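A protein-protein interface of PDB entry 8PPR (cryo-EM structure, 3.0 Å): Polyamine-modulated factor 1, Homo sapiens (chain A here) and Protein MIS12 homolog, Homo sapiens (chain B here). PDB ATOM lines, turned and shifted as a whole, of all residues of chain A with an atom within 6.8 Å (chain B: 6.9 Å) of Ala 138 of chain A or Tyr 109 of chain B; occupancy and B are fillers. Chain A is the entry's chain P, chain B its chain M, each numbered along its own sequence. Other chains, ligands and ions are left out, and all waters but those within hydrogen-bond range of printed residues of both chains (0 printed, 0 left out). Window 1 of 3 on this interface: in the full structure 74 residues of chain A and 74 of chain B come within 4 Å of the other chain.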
ATOM      1  N   LYS A 131      17.469   3.615  -5.994  1.00  0.00           N
ATOM      2  CA  LYS A 131      18.208   3.002  -7.090  1.00  0.00           C
ATOM      3  C   LYS A 131      19.610   2.598  -6.659  1.00  0.00           C
ATOM      4  O   LYS A 131      20.169   1.636  -7.197  1.00  0.00           O
ATOM      5  CB  LYS A 131      18.260   3.951  -8.285  1.00  0.00           C
ATOM      6  CG  LYS A 131      17.212   3.651  -9.344  1.00  0.00           C
ATOM      7  CD  LYS A 131      15.801   3.764  -8.786  1.00  0.00           C
ATOM      8  CE  LYS A 131      15.425   5.205  -8.499  1.00  0.00           C
ATOM      9  NZ  LYS A 131      13.996   5.337  -8.106  1.00  0.00           N
ATOM     10  N   LEU A 133      20.350   1.387  -3.657  1.00  0.00           N
ATOM     11  CA  LEU A 133      20.163   0.171  -2.878  1.00  0.00           C
ATOM     12  C   LEU A 133      19.610  -0.984  -3.699  1.00  0.00           C
ATOM     13  O   LEU A 133      19.677  -2.135  -3.247  1.00  0.00           O
ATOM     14  CB  LEU A 133      19.222   0.451  -1.700  1.00  0.00           C
ATOM     15  CG  LEU A 133      19.820   1.187  -0.498  1.00  0.00           C
ATOM     16  CD1 LEU A 133      18.870   1.143   0.687  1.00  0.00           C
ATOM     17  CD2 LEU A 133      21.169   0.596  -0.125  1.00  0.00           C
ATOM     18  N   HIS A 134      19.056  -0.698  -4.879  1.00  0.00           N
ATOM     19  CA  HIS A 134      18.519  -1.760  -5.722  1.00  0.00           C
ATOM     20  C   HIS A 134      19.602  -2.756  -6.113  1.00  0.00           C
ATOM     21  O   HIS A 134      19.387  -3.972  -6.059  1.00  0.00           O
ATOM     22  CB  HIS A 134      17.873  -1.154  -6.968  1.00  0.00           C
ATOM     23  CG  HIS A 134      16.486  -0.642  -6.740  1.00  0.00           C
ATOM     24  ND1 HIS A 134      15.737  -0.988  -5.636  1.00  0.00           N
ATOM     25  CD2 HIS A 134      15.716   0.202  -7.467  1.00  0.00           C
ATOM     26  CE1 HIS A 134      14.563  -0.386  -5.697  1.00  0.00           C
ATOM     27  NE2 HIS A 134      14.525   0.343  -6.797  1.00  0.00           N
ATOM     28  N   SER A 135      20.779  -2.258  -6.503  1.00  0.00           N
ATOM     29  CA  SER A 135      21.876  -3.151  -6.863  1.00  0.00           C
ATOM     30  C   SER A 135      22.316  -3.991  -5.672  1.00  0.00           C
ATOM     31  O   SER A 135      22.645  -5.173  -5.823  1.00  0.00           O
ATOM     32  CB  SER A 135      23.054  -2.343  -7.409  1.00  0.00           C
ATOM     33  OG  SER A 135      24.265  -3.067  -7.286  1.00  0.00           O
ATOM     34  N   VAL A 136      22.340  -3.392  -4.482  1.00  0.00           N
ATOM     35  CA  VAL A 136      22.775  -4.117  -3.294  1.00  0.00           C
ATOM     36  C   VAL A 136      21.806  -5.242  -2.962  1.00  0.00           C
ATOM     37  O   VAL A 136      22.218  -6.376  -2.691  1.00  0.00           O
ATOM     38  CB  VAL A 136      22.933  -3.144  -2.112  1.00  0.00           C
ATOM     39  CG1 VAL A 136      22.980  -3.908  -0.795  1.00  0.00           C
ATOM     40  CG2 VAL A 136      24.177  -2.290  -2.295  1.00  0.00           C
ATOM     41  N   MET A 137      20.507  -4.955  -2.979  1.00  0.00           N
ATOM     42  CA  MET A 137      19.528  -5.921  -2.498  1.00  0.00           C
ATOM     43  C   MET A 137      18.935  -6.800  -3.594  1.00  0.00           C
ATOM     44  O   MET A 137      18.115  -7.671  -3.283  1.00  0.00           O
ATOM     45  CB  MET A 137      18.419  -5.197  -1.724  1.00  0.00           C
ATOM     46  CG  MET A 137      17.553  -4.249  -2.532  1.00  0.00           C
ATOM     47  SD  MET A 137      16.341  -3.436  -1.469  1.00  0.00           S
ATOM     48  CE  MET A 137      15.489  -2.377  -2.634  1.00  0.00           C
ATOM     49  N   ALA A 138      19.323  -6.612  -4.856  1.00  0.00           N
ATOM     50  CA  ALA A 138      18.854  -7.517  -5.904  1.00  0.00           C
ATOM     51  C   ALA A 138      19.316  -8.962  -5.726  1.00  0.00           C
ATOM     52  O   ALA A 138      18.465  -9.867  -5.810  1.00  0.00           O
ATOM     53  CB  ALA A 138      19.274  -6.966  -7.271  1.00  0.00           C
ATOM     54  N   PRO A 139      20.607  -9.259  -5.501  1.00  0.00           N
ATOM     55  CA  PRO A 139      21.036 -10.672  -5.532  1.00  0.00           C
ATOM     56  C   PRO A 139      20.341 -11.557  -4.513  1.00  0.00           C
ATOM     57  O   PRO A 139      20.050 -12.725  -4.803  1.00  0.00           O
ATOM     58  CB  PRO A 139      22.544 -10.580  -5.256  1.00  0.00           C
ATOM     59  CG  PRO A 139      22.924  -9.209  -5.676  1.00  0.00           C
ATOM     60  CD  PRO A 139      21.756  -8.359  -5.289  1.00  0.00           C
ATOM     61  N   TYR A 140      20.067 -11.035  -3.320  1.00  0.00           N
ATOM     62  CA  TYR A 140      19.451 -11.863  -2.290  1.00  0.00           C
ATOM     63  C   TYR A 140      17.993 -12.152  -2.622  1.00  0.00           C
ATOM     64  O   TYR A 140      17.497 -13.257  -2.371  1.00  0.00           O
ATOM     65  CB  TYR A 140      19.588 -11.177  -0.935  1.00  0.00           C
ATOM     66  CG  TYR A 140      21.018 -11.120  -0.454  1.00  0.00           C
ATOM     67  CD1 TYR A 140      22.001 -11.904  -1.043  1.00  0.00           C
ATOM     68  CD2 TYR A 140      21.392 -10.266   0.568  1.00  0.00           C
ATOM     69  CE1 TYR A 140      23.311 -11.853  -0.611  1.00  0.00           C
ATOM     70  CE2 TYR A 140      22.697 -10.209   1.010  1.00  0.00           C
ATOM     71  CZ  TYR A 140      23.653 -11.000   0.415  1.00  0.00           C
ATOM     72  OH  TYR A 140      24.956 -10.939   0.853  1.00  0.00           O
ATOM     73  N   PHE A 141      17.298 -11.173  -3.203  1.00  0.00           N
ATOM     74  CA  PHE A 141      15.954 -11.428  -3.706  1.00  0.00           C
ATOM     75  C   PHE A 141      15.981 -12.464  -4.818  1.00  0.00           C
ATOM     76  O   PHE A 141      15.087 -13.314  -4.907  1.00  0.00           O
ATOM     77  CB  PHE A 141      15.322 -10.127  -4.196  1.00  0.00           C
ATOM     78  CG  PHE A 141      14.657  -9.334  -3.115  1.00  0.00           C
ATOM     79  CD1 PHE A 141      15.408  -8.604  -2.212  1.00  0.00           C
ATOM     80  CD2 PHE A 141      13.279  -9.322  -2.996  1.00  0.00           C
ATOM     81  CE1 PHE A 141      14.798  -7.872  -1.214  1.00  0.00           C
ATOM     82  CE2 PHE A 141      12.663  -8.595  -1.999  1.00  0.00           C
ATOM     83  CZ  PHE A 141      13.423  -7.867  -1.107  1.00  0.00           C
ATOM     84  N   LEU A 142      17.000 -12.411  -5.679  1.00  0.00           N
ATOM     85  CA  LEU A 142      17.138 -13.426  -6.719  1.00  0.00           C
ATOM     86  C   LEU A 142      17.322 -14.811  -6.113  1.00  0.00           C
ATOM     87  O   LEU A 142      16.717 -15.787  -6.573  1.00  0.00           O
ATOM     88  CB  LEU A 142      18.317 -13.081  -7.628  1.00  0.00           C
ATOM     89  CG  LEU A 142      18.104 -11.950  -8.632  1.00  0.00           C
ATOM     90  CD1 LEU A 142      19.174 -11.989  -9.710  1.00  0.00           C
ATOM     91  CD2 LEU A 142      16.720 -12.038  -9.251  1.00  0.00           C
ATOM     92  N   GLN A 143      18.157 -14.911  -5.078  1.00  0.00           N
ATOM     93  CA  GLN A 143      18.367 -16.191  -4.406  1.00  0.00           C
ATOM     94  C   GLN A 143      17.078 -16.708  -3.780  1.00  0.00           C
ATOM     95  O   GLN A 143      16.758 -17.902  -3.883  1.00  0.00           O
ATOM     96  CB  GLN A 143      19.453 -16.039  -3.343  1.00  0.00           C
ATOM     97  CG  GLN A 143      19.559 -17.208  -2.386  1.00  0.00           C
ATOM     98  CD  GLN A 143      20.133 -16.804  -1.044  1.00  0.00           C
ATOM     99  OE1 GLN A 143      19.432 -16.801  -0.032  1.00  0.00           O
ATOM    100  NE2 GLN A 143      21.413 -16.452  -1.029  1.00  0.00           N
ATOM    101  N   ARG A 145      14.016 -15.991  -4.719  1.00  0.00           N
ATOM    102  CA  ARG A 145      13.152 -16.406  -5.816  1.00  0.00           C
ATOM    103  C   ARG A 145      13.550 -17.778  -6.338  1.00  0.00           C
ATOM    104  O   ARG A 145      12.687 -18.615  -6.622  1.00  0.00           O
ATOM    105  CB  ARG A 145      13.210 -15.375  -6.940  1.00  0.00           C
ATOM    106  CG  ARG A 145      12.450 -15.778  -8.186  1.00  0.00           C
ATOM    107  CD  ARG A 145      12.842 -14.897  -9.352  1.00  0.00           C
ATOM    108  NE  ARG A 145      14.217 -15.147  -9.767  1.00  0.00           N
ATOM    109  CZ  ARG A 145      14.789 -14.604 -10.832  1.00  0.00           C
ATOM    110  NH1 ARG A 145      14.131 -13.768 -11.619  1.00  0.00           N
ATOM    111  NH2 ARG A 145      16.053 -14.906 -11.115  1.00  0.00           N
ATOM    112  N   THR B 107      27.418  -3.893 -11.492  1.00  0.00           N
ATOM    113  CA  THR B 107      26.375  -4.205 -12.462  1.00  0.00           C
ATOM    114  C   THR B 107      25.112  -3.405 -12.160  1.00  0.00           C
ATOM    115  O   THR B 107      24.631  -3.417 -11.020  1.00  0.00           O
ATOM    116  CB  THR B 107      26.069  -5.701 -12.482  1.00  0.00           C
ATOM    117  OG1 THR B 107      25.035  -5.970 -13.438  1.00  0.00           O
ATOM    118  CG2 THR B 107      25.666  -6.220 -11.102  1.00  0.00           C
ATOM    119  N   PRO B 108      24.581  -2.664 -13.129  1.00  0.00           N
ATOM    120  CA  PRO B 108      23.326  -1.945 -12.903  1.00  0.00           C
ATOM    121  C   PRO B 108      22.141  -2.896 -12.840  1.00  0.00           C
ATOM    122  O   PRO B 108      22.153  -3.996 -13.395  1.00  0.00           O
ATOM    123  CB  PRO B 108      23.224  -1.014 -14.116  1.00  0.00           C
ATOM    124  CG  PRO B 108      24.004  -1.709 -15.178  1.00  0.00           C
ATOM    125  CD  PRO B 108      25.125  -2.426 -14.477  1.00  0.00           C
ATOM    126  N   TYR B 109      21.100  -2.447 -12.142  1.00  0.00           N
ATOM    127  CA  TYR B 109      19.846  -3.187 -12.038  1.00  0.00           C
ATOM    128  C   TYR B 109      18.702  -2.192 -12.159  1.00  0.00           C
ATOM    129  O   TYR B 109      18.525  -1.339 -11.285  1.00  0.00           O
ATOM    130  CB  TYR B 109      19.762  -3.965 -10.727  1.00  0.00           C
ATOM    131  CG  TYR B 109      18.747  -5.083 -10.757  1.00  0.00           C
ATOM    132  CD1 TYR B 109      17.397  -4.821 -10.579  1.00  0.00           C
ATOM    133  CD2 TYR B 109      19.135  -6.398 -10.978  1.00  0.00           C
ATOM    134  CE1 TYR B 109      16.465  -5.834 -10.608  1.00  0.00           C
ATOM    135  CE2 TYR B 109      18.205  -7.420 -11.012  1.00  0.00           C
ATOM    136  CZ  TYR B 109      16.870  -7.130 -10.827  1.00  0.00           C
ATOM    137  OH  TYR B 109      15.934  -8.139 -10.858  1.00  0.00           O
ATOM    138  N   SER B 110      17.932  -2.301 -13.238  1.00  0.00           N
ATOM    139  CA  SER B 110      16.842  -1.368 -13.472  1.00  0.00           C
ATOM    140  C   SER B 110      15.735  -1.556 -12.441  1.00  0.00           C
ATOM    141  O   SER B 110      15.511  -2.654 -11.924  1.00  0.00           O
ATOM    142  CB  SER B 110      16.276  -1.548 -14.880  1.00  0.00           C
ATOM    143  OG  SER B 110      15.611  -2.789 -15.004  1.00  0.00           O
ATOM    144  N   GLU B 111      15.040  -0.456 -12.147  1.00  0.00           N
ATOM    145  CA  GLU B 111      13.940  -0.501 -11.189  1.00  0.00           C
ATOM    146  C   GLU B 111      12.806  -1.387 -11.689  1.00  0.00           C
ATOM    147  O   GLU B 111      12.152  -2.074 -10.894  1.00  0.00           O
ATOM    148  CB  GLU B 111      13.436   0.915 -10.911  1.00  0.00           C
ATOM    149  CG  GLU B 111      12.480   1.021  -9.735  1.00  0.00           C
ATOM    150  CD  GLU B 111      11.041   0.754 -10.133  1.00  0.00           C
ATOM    151  OE1 GLU B 111      10.692   1.007 -11.306  1.00  0.00           O
ATOM    152  OE2 GLU B 111      10.261   0.287  -9.277  1.00  0.00           O
ATOM    153  N   GLU B 112      12.546  -1.372 -12.997  1.00  0.00           N
ATOM    154  CA  GLU B 112      11.480  -2.202 -13.546  1.00  0.00           C
ATOM    155  C   GLU B 112      11.768  -3.681 -13.332  1.00  0.00           C
ATOM    156  O   GLU B 112      10.861  -4.457 -13.009  1.00  0.00           O
ATOM    157  CB  GLU B 112      11.290  -1.905 -15.033  1.00  0.00           C
ATOM    158  CG  GLU B 112      10.060  -2.564 -15.630  1.00  0.00           C
ATOM    159  CD  GLU B 112       8.870  -2.532 -14.691  1.00  0.00           C
ATOM    160  OE1 GLU B 112       8.465  -1.424 -14.278  1.00  0.00           O
ATOM    161  OE2 GLU B 112       8.344  -3.615 -14.358  1.00  0.00           O
ATOM    162  N   ASP B 113      13.024  -4.090 -13.515  1.00  0.00           N
ATOM    163  CA  ASP B 113      13.392  -5.475 -13.248  1.00  0.00           C
ATOM    164  C   ASP B 113      13.175  -5.821 -11.784  1.00  0.00           C
ATOM    165  O   ASP B 113      12.727  -6.925 -11.458  1.00  0.00           O
ATOM    166  CB  ASP B 113      14.846  -5.719 -13.644  1.00  0.00           C
ATOM    167  CG  ASP B 113      15.052  -5.685 -15.138  1.00  0.00           C
ATOM    168  OD1 ASP B 113      14.061  -5.860 -15.876  1.00  0.00           O
ATOM    169  OD2 ASP B 113      16.201  -5.469 -15.575  1.00  0.00           O
ATOM    170  N   PHE B 114      13.489  -4.888 -10.883  1.00  0.00           N
ATOM    171  CA  PHE B 114      13.286  -5.135  -9.461  1.00  0.00           C
ATOM    172  C   PHE B 114      11.806  -5.292  -9.134  1.00  0.00           C
ATOM    173  O   PHE B 114      11.419  -6.167  -8.351  1.00  0.00           O
ATOM    174  CB  PHE B 114      13.911  -4.008  -8.641  1.00  0.00           C
ATOM    175  CG  PHE B 114      14.128  -4.365  -7.204  1.00  0.00           C
ATOM    176  CD1 PHE B 114      15.212  -5.138  -6.828  1.00  0.00           C
ATOM    177  CD2 PHE B 114      13.248  -3.932  -6.229  1.00  0.00           C
ATOM    178  CE1 PHE B 114      15.415  -5.474  -5.508  1.00  0.00           C
ATOM    179  CE2 PHE B 114      13.447  -4.263  -4.906  1.00  0.00           C
ATOM    180  CZ  PHE B 114      14.530  -5.038  -4.545  1.00  0.00           C
ATOM    181  N   GLN B 115      10.960  -4.445  -9.724  1.00  0.00           N
ATOM    182  CA  GLN B 115       9.522  -4.565  -9.503  1.00  0.00           C
ATOM    183  C   GLN B 115       8.987  -5.880 -10.056  1.00  0.00           C
ATOM    184  O   GLN B 115       8.162  -6.545  -9.415  1.00  0.00           O
ATOM    185  CB  GLN B 115       8.796  -3.379 -10.136  1.00  0.00           C
ATOM    186  CG  GLN B 115       7.304  -3.363  -9.869  1.00  0.00           C
ATOM    187  CD  GLN B 115       6.973  -3.674  -8.425  1.00  0.00           C
ATOM    188  OE1 GLN B 115       6.357  -4.697  -8.126  1.00  0.00           O
ATOM    189  NE2 GLN B 115       7.386  -2.795  -7.519  1.00  0.00           N
ATOM    190  N   HIS B 116       9.451  -6.271 -11.244  1.00  0.00           N
ATOM    191  CA  HIS B 116       9.062  -7.559 -11.805  1.00  0.00           C
ATOM    192  C   HIS B 116       9.495  -8.704 -10.903  1.00  0.00           C
ATOM    193  O   HIS B 116       8.751  -9.671 -10.713  1.00  0.00           O
ATOM    194  CB  HIS B 116       9.663  -7.725 -13.198  1.00  0.00           C
ATOM    195  CG  HIS B 116       9.596  -9.127 -13.713  1.00  0.00           C
ATOM    196  ND1 HIS B 116       8.412  -9.821 -13.829  1.00  0.00           N
ATOM    197  CD2 HIS B 116      10.570  -9.971 -14.128  1.00  0.00           C
ATOM    198  CE1 HIS B 116       8.658 -11.030 -14.302  1.00  0.00           C
ATOM    199  NE2 HIS B 116       9.959 -11.146 -14.491  1.00  0.00           N
ATOM    200  N   LEU B 117      10.703  -8.614 -10.349  1.00  0.00           N
ATOM    201  CA  LEU B 117      11.193  -9.647  -9.446  1.00  0.00           C
ATOM    202  C   LEU B 117      10.348  -9.723  -8.180  1.00  0.00           C
ATOM    203  O   LEU B 117      10.045 -10.819  -7.695  1.00  0.00           O
ATOM    204  CB  LEU B 117      12.659  -9.376  -9.112  1.00  0.00           C
ATOM    205  CG  LEU B 117      13.252 -10.024  -7.865  1.00  0.00           C
ATOM    206  CD1 LEU B 117      13.302 -11.533  -8.019  1.00  0.00           C
ATOM    207  CD2 LEU B 117      14.639  -9.462  -7.619  1.00  0.00           C
ATOM    208  N   GLN B 118       9.962  -8.570  -7.632  1.00  0.00           N
ATOM    209  CA  GLN B 118       9.089  -8.560  -6.462  1.00  0.00           C
ATOM    210  C   GLN B 118       7.755  -9.223  -6.776  1.00  0.00           C
ATOM    211  O   GLN B 118       7.247 -10.040  -5.994  1.00  0.00           O
ATOM    212  CB  GLN B 118       8.869  -7.125  -5.983  1.00  0.00           C
ATOM    213  CG  GLN B 118      10.108  -6.433  -5.443  1.00  0.00           C
ATOM    214  CD  GLN B 118      10.378  -6.766  -3.991  1.00  0.00           C
ATOM    215  OE1 GLN B 118       9.671  -7.571  -3.384  1.00  0.00           O
ATOM    216  NE2 GLN B 118      11.392  -6.131  -3.419  1.00  0.00           N
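O of Asp 113 of chain B lies within hydrogen-bond range of OH of Tyr 109 of chain B (3.5 Å).
Of the printed residues of chain B, Arg 145 of chain A touches Leu 117. Tyr 109 of chain B touches just one residue of chain A: Ala 138. Ser 110 of chain B touches none of the printed residues of chain A. Printed residues of chain A within 4 Å of Phe 114 of chain B: His 134 (3.8 Å) and Met 137 (3.4 Å). The nearest printed residue of chain A that does not touch Glu 111 of chain B is Lys 131 of chain A (4.3 Å).
Printed residues of chain A that touch a printed residue of chain B: His 134, Ser 135, Met 137, Ala 138, Phe 141, Leu 142 and Arg 145. Hydrophobic or aromatic side chains of chain A that line the printed part of chain B: His 134, Met 137, Ala 138, Phe 141 and Leu 142. Hydrophobic or aromatic side chains of chain B that line the printed part of chain A: Tyr 109, Phe 114 and Leu 117. Among the printed residues, 9 pairs touch across the chains. Among the printed residues, no Asp or Glu carboxylate lies within 4 Å of a Lys or Arg side-chain nitrogen of the other chain.
Among the printed residues, pairs that only touch across the chains: Phe 141 of chain A with Gln 118 of chain B, Met 137 of chain A with Phe 114 of chain B, Phe 141 of chain A with Leu 117 of chain B, His 134 of chain A with Glu 111 of chain B, Arg 145 of chain A with Leu 117 of chain B, Leu 142 of chain A with Leu 117 of chain B, Ala 138 of chain A with Tyr 109 of chain B, Ser 135 of chain A with Thr 107 of chain B and His 134 of chain A with Phe 114 of chain B.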
